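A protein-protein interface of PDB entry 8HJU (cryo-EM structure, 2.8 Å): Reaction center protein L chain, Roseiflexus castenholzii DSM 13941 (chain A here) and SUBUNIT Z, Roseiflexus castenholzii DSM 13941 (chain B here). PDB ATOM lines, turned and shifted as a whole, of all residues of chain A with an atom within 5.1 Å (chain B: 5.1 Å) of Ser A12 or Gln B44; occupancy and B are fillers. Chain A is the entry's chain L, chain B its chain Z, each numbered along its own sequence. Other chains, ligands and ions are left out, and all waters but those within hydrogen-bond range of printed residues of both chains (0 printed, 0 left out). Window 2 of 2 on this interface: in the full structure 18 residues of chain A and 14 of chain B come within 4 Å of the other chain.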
ATOM      1  N   LEU A  10     -22.146   0.560  -6.307  1.00  0.00           N
ATOM      2  CA  LEU A  10     -22.545   1.684  -5.475  1.00  0.00           C
ATOM      3  C   LEU A  10     -22.425   1.347  -3.997  1.00  0.00           C
ATOM      4  O   LEU A  10     -22.281   0.185  -3.613  1.00  0.00           O
ATOM      5  CB  LEU A  10     -23.980   2.088  -5.797  1.00  0.00           C
ATOM      6  CG  LEU A  10     -24.292   2.644  -7.180  1.00  0.00           C
ATOM      7  CD1 LEU A  10     -25.753   2.978  -7.261  1.00  0.00           C
ATOM      8  CD2 LEU A  10     -23.477   3.871  -7.431  1.00  0.00           C
ATOM      9  N   PRO A  11     -22.476   2.359  -3.129  1.00  0.00           N
ATOM     10  CA  PRO A  11     -22.407   2.088  -1.686  1.00  0.00           C
ATOM     11  C   PRO A  11     -23.534   1.219  -1.170  1.00  0.00           C
ATOM     12  O   PRO A  11     -23.341   0.484  -0.197  1.00  0.00           O
ATOM     13  CB  PRO A  11     -22.452   3.492  -1.075  1.00  0.00           C
ATOM     14  CG  PRO A  11     -21.915   4.363  -2.122  1.00  0.00           C
ATOM     15  CD  PRO A  11     -22.385   3.796  -3.416  1.00  0.00           C
ATOM     16  N   SER A  12     -24.717   1.291  -1.773  1.00  0.00           N
ATOM     17  CA  SER A  12     -25.830   0.494  -1.278  1.00  0.00           C
ATOM     18  C   SER A  12     -25.627  -0.985  -1.579  1.00  0.00           C
ATOM     19  O   SER A  12     -26.022  -1.850  -0.791  1.00  0.00           O
ATOM     20  CB  SER A  12     -27.136   1.000  -1.878  1.00  0.00           C
ATOM     21  OG  SER A  12     -27.120   0.926  -3.284  1.00  0.00           O
ATOM     22  N   GLY A  13     -25.000  -1.296  -2.705  1.00  0.00           N
ATOM     23  CA  GLY A  13     -24.823  -2.676  -3.100  1.00  0.00           C
ATOM     24  C   GLY A  13     -25.368  -2.867  -4.490  1.00  0.00           C
ATOM     25  O   GLY A  13     -25.178  -3.902  -5.125  1.00  0.00           O
ATOM     26  N   GLU A  14     -26.072  -1.847  -4.956  1.00  0.00           N
ATOM     27  CA  GLU A  14     -26.552  -1.826  -6.324  1.00  0.00           C
ATOM     28  C   GLU A  14     -25.399  -1.605  -7.289  1.00  0.00           C
ATOM     29  O   GLU A  14     -24.524  -0.771  -7.056  1.00  0.00           O
ATOM     30  CB  GLU A  14     -27.578  -0.717  -6.495  1.00  0.00           C
ATOM     31  CG  GLU A  14     -28.956  -1.200  -6.837  1.00  0.00           C
ATOM     32  CD  GLU A  14     -29.917  -0.057  -7.047  1.00  0.00           C
ATOM     33  OE1 GLU A  14     -31.030  -0.309  -7.548  1.00  0.00           O
ATOM     34  OE2 GLU A  14     -29.560   1.092  -6.713  1.00  0.00           O
ATOM     35  N   LYS A 238     -32.821   2.662  -3.186  1.00  0.00           N
ATOM     36  CA  LYS A 238     -32.360   2.151  -4.472  1.00  0.00           C
ATOM     37  C   LYS A 238     -33.367   2.468  -5.567  1.00  0.00           C
ATOM     38  O   LYS A 238     -33.727   1.625  -6.388  1.00  0.00           O
ATOM     39  CB  LYS A 238     -32.085   0.656  -4.364  1.00  0.00           C
ATOM     40  CG  LYS A 238     -30.939   0.338  -3.422  1.00  0.00           C
ATOM     41  CD  LYS A 238     -31.189  -0.916  -2.618  1.00  0.00           C
ATOM     42  CE  LYS A 238     -30.765  -2.148  -3.381  1.00  0.00           C
ATOM     43  NZ  LYS A 238     -30.725  -3.342  -2.493  1.00  0.00           N
ATOM     44  N   PHE B  40     -21.221  -8.985   7.764  1.00  0.00           N
ATOM     45  CA  PHE B  40     -21.675  -8.611   6.431  1.00  0.00           C
ATOM     46  C   PHE B  40     -21.840  -7.107   6.282  1.00  0.00           C
ATOM     47  O   PHE B  40     -21.568  -6.560   5.203  1.00  0.00           O
ATOM     48  CB  PHE B  40     -22.963  -9.355   6.106  1.00  0.00           C
ATOM     49  CG  PHE B  40     -22.722 -10.755   5.654  1.00  0.00           C
ATOM     50  CD1 PHE B  40     -22.117 -11.010   4.438  1.00  0.00           C
ATOM     51  CD2 PHE B  40     -23.052 -11.816   6.461  1.00  0.00           C
ATOM     52  CE1 PHE B  40     -21.878 -12.300   4.030  1.00  0.00           C
ATOM     53  CE2 PHE B  40     -22.813 -13.100   6.062  1.00  0.00           C
ATOM     54  CZ  PHE B  40     -22.227 -13.346   4.846  1.00  0.00           C
ATOM     55  N   THR B  41     -22.236  -6.428   7.356  1.00  0.00           N
ATOM     56  CA  THR B  41     -22.203  -4.978   7.380  1.00  0.00           C
ATOM     57  C   THR B  41     -20.840  -4.471   6.952  1.00  0.00           C
ATOM     58  O   THR B  41     -20.738  -3.633   6.052  1.00  0.00           O
ATOM     59  CB  THR B  41     -22.535  -4.477   8.787  1.00  0.00           C
ATOM     60  OG1 THR B  41     -23.830  -4.941   9.172  1.00  0.00           O
ATOM     61  CG2 THR B  41     -22.524  -2.979   8.850  1.00  0.00           C
ATOM     62  N   ASP B  42     -19.775  -5.012   7.534  1.00  0.00           N
ATOM     63  CA  ASP B  42     -18.471  -4.476   7.194  1.00  0.00           C
ATOM     64  C   ASP B  42     -17.929  -5.022   5.885  1.00  0.00           C
ATOM     65  O   ASP B  42     -17.141  -4.341   5.232  1.00  0.00           O
ATOM     66  CB  ASP B  42     -17.462  -4.714   8.301  1.00  0.00           C
ATOM     67  CG  ASP B  42     -16.348  -3.693   8.261  1.00  0.00           C
ATOM     68  OD1 ASP B  42     -16.382  -2.849   7.345  1.00  0.00           O
ATOM     69  OD2 ASP B  42     -15.455  -3.709   9.128  1.00  0.00           O
ATOM     70  N   LYS B  43     -18.287  -6.236   5.479  1.00  0.00           N
ATOM     71  CA  LYS B  43     -17.919  -6.620   4.124  1.00  0.00           C
ATOM     72  C   LYS B  43     -18.445  -5.608   3.121  1.00  0.00           C
ATOM     73  O   LYS B  43     -17.701  -5.147   2.246  1.00  0.00           O
ATOM     74  CB  LYS B  43     -18.430  -8.013   3.799  1.00  0.00           C
ATOM     75  CG  LYS B  43     -17.399  -9.074   4.022  1.00  0.00           C
ATOM     76  CD  LYS B  43     -17.374 -10.034   2.870  1.00  0.00           C
ATOM     77  CE  LYS B  43     -18.768 -10.289   2.377  1.00  0.00           C
ATOM     78  NZ  LYS B  43     -18.778 -11.316   1.312  1.00  0.00           N
ATOM     79  N   GLN B  44     -19.710  -5.211   3.259  1.00  0.00           N
ATOM     80  CA  GLN B  44     -20.249  -4.209   2.349  1.00  0.00           C
ATOM     81  C   GLN B  44     -19.568  -2.860   2.542  1.00  0.00           C
ATOM     82  O   GLN B  44     -19.229  -2.190   1.564  1.00  0.00           O
ATOM     83  CB  GLN B  44     -21.759  -4.089   2.529  1.00  0.00           C
ATOM     84  CG  GLN B  44     -22.445  -3.124   1.574  1.00  0.00           C
ATOM     85  CD  GLN B  44     -21.997  -3.268   0.132  1.00  0.00           C
ATOM     86  OE1 GLN B  44     -21.484  -4.309  -0.259  1.00  0.00           O
ATOM     87  NE2 GLN B  44     -22.165  -2.218  -0.657  1.00  0.00           N
ATOM     88  N   ALA B  45     -19.339  -2.452   3.789  1.00  0.00           N
ATOM     89  CA  ALA B  45     -18.814  -1.115   4.031  1.00  0.00           C
ATOM     90  C   ALA B  45     -17.364  -0.969   3.589  1.00  0.00           C
ATOM     91  O   ALA B  45     -16.951   0.125   3.198  1.00  0.00           O
ATOM     92  CB  ALA B  45     -18.950  -0.762   5.505  1.00  0.00           C
ATOM     93  N   THR B  46     -16.573  -2.034   3.658  1.00  0.00           N
ATOM     94  CA  THR B  46     -15.181  -1.986   3.248  1.00  0.00           C
ATOM     95  C   THR B  46     -14.966  -2.480   1.830  1.00  0.00           C
ATOM     96  O   THR B  46     -13.829  -2.467   1.357  1.00  0.00           O
ATOM     97  CB  THR B  46     -14.312  -2.807   4.199  1.00  0.00           C
ATOM     98  OG1 THR B  46     -14.796  -4.152   4.247  1.00  0.00           O
ATOM     99  CG2 THR B  46     -14.331  -2.210   5.585  1.00  0.00           C
ATOM    100  N   SER B  47     -16.015  -2.922   1.143  1.00  0.00           N
ATOM    101  CA  SER B  47     -15.854  -3.220  -0.268  1.00  0.00           C
ATOM    102  C   SER B  47     -15.573  -1.938  -1.050  1.00  0.00           C
ATOM    103  O   SER B  47     -15.661  -0.824  -0.531  1.00  0.00           O
ATOM    104  CB  SER B  47     -17.092  -3.922  -0.814  1.00  0.00           C
ATOM    105  OG  SER B  47     -18.221  -3.079  -0.748  1.00  0.00           O
ATOM    106  N   TYR B  49     -16.560   0.662  -3.837  1.00  0.00           N
ATOM    107  CA  TYR B  49     -17.695   1.194  -4.565  1.00  0.00           C
ATOM    108  C   TYR B  49     -17.447   2.676  -4.795  1.00  0.00           C
ATOM    109  O   TYR B  49     -16.416   3.218  -4.397  1.00  0.00           O
ATOM    110  CB  TYR B  49     -19.004   0.937  -3.820  1.00  0.00           C
ATOM    111  CG  TYR B  49     -18.980   1.272  -2.353  1.00  0.00           C
ATOM    112  CD1 TYR B  49     -18.951   2.583  -1.927  1.00  0.00           C
ATOM    113  CD2 TYR B  49     -19.018   0.279  -1.397  1.00  0.00           C
ATOM    114  CE1 TYR B  49     -18.942   2.892  -0.605  1.00  0.00           C
ATOM    115  CE2 TYR B  49     -19.009   0.581  -0.069  1.00  0.00           C
ATOM    116  CZ  TYR B  49     -18.971   1.890   0.323  1.00  0.00           C
ATOM    117  OH  TYR B  49     -18.962   2.210   1.654  1.00  0.00           O
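The side-chain hydroxyl (OG) of Ser A12 sits at hydrogen-bond distance from the backbone NH (N) of Glu A14 (3.4 Å). OG of Ser B47 sits at hydrogen-bond distance from O of Gln B44, 2.7 Å away. The backbone carbonyl oxygen of Ala B45 sits at hydrogen-bond distance from the side-chain hydroxyl of Tyr B49 (3.3 Å).
Printed residues of chain B within 4 Å of Leu A10: Gln B44 and Tyr B49. Of chain B, only Gln B44 comes within 4 Å of Ser A12. Of the printed residues of chain B, Gly A13 touches Gln B44 (3.6 Å). Phe B40 touches none of the printed residues of chain A. Of chain A, only Leu A10, Pro A11, Ser A12 and Gly A13 come within 4 Å of Gln B44. Ser B47 touches none of the printed residues of chain A. Of the printed residues of chain A, Tyr B49 touches Leu A10 (3.4 Å) and Pro A11 (3.5 Å). The nearest printed residue of chain A that does not touch Gln B44 is Glu A14 (5.8 Å).
NE2 of Gln B44 sits at hydrogen-bond distance from O of Pro A11 (3.0 Å).
Among the printed residues, merely in contact across the chains: Leu A10 with Gln B44, Leu A10 with Tyr B49, Pro A11 with Tyr B49, Ser A12 with Gln B44 and Gly A13 with Gln B44.
Of the 9 printed residues of chain B, 2 touch a printed residue of chain A. Hydrophobic or aromatic side chains of chain B that line the printed part of chain A: Tyr B49. Hydrophobic or aromatic side chains of chain A that line the printed part of chain B: Pro A11. Among the printed residues, 6 pairs touch across the chains.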
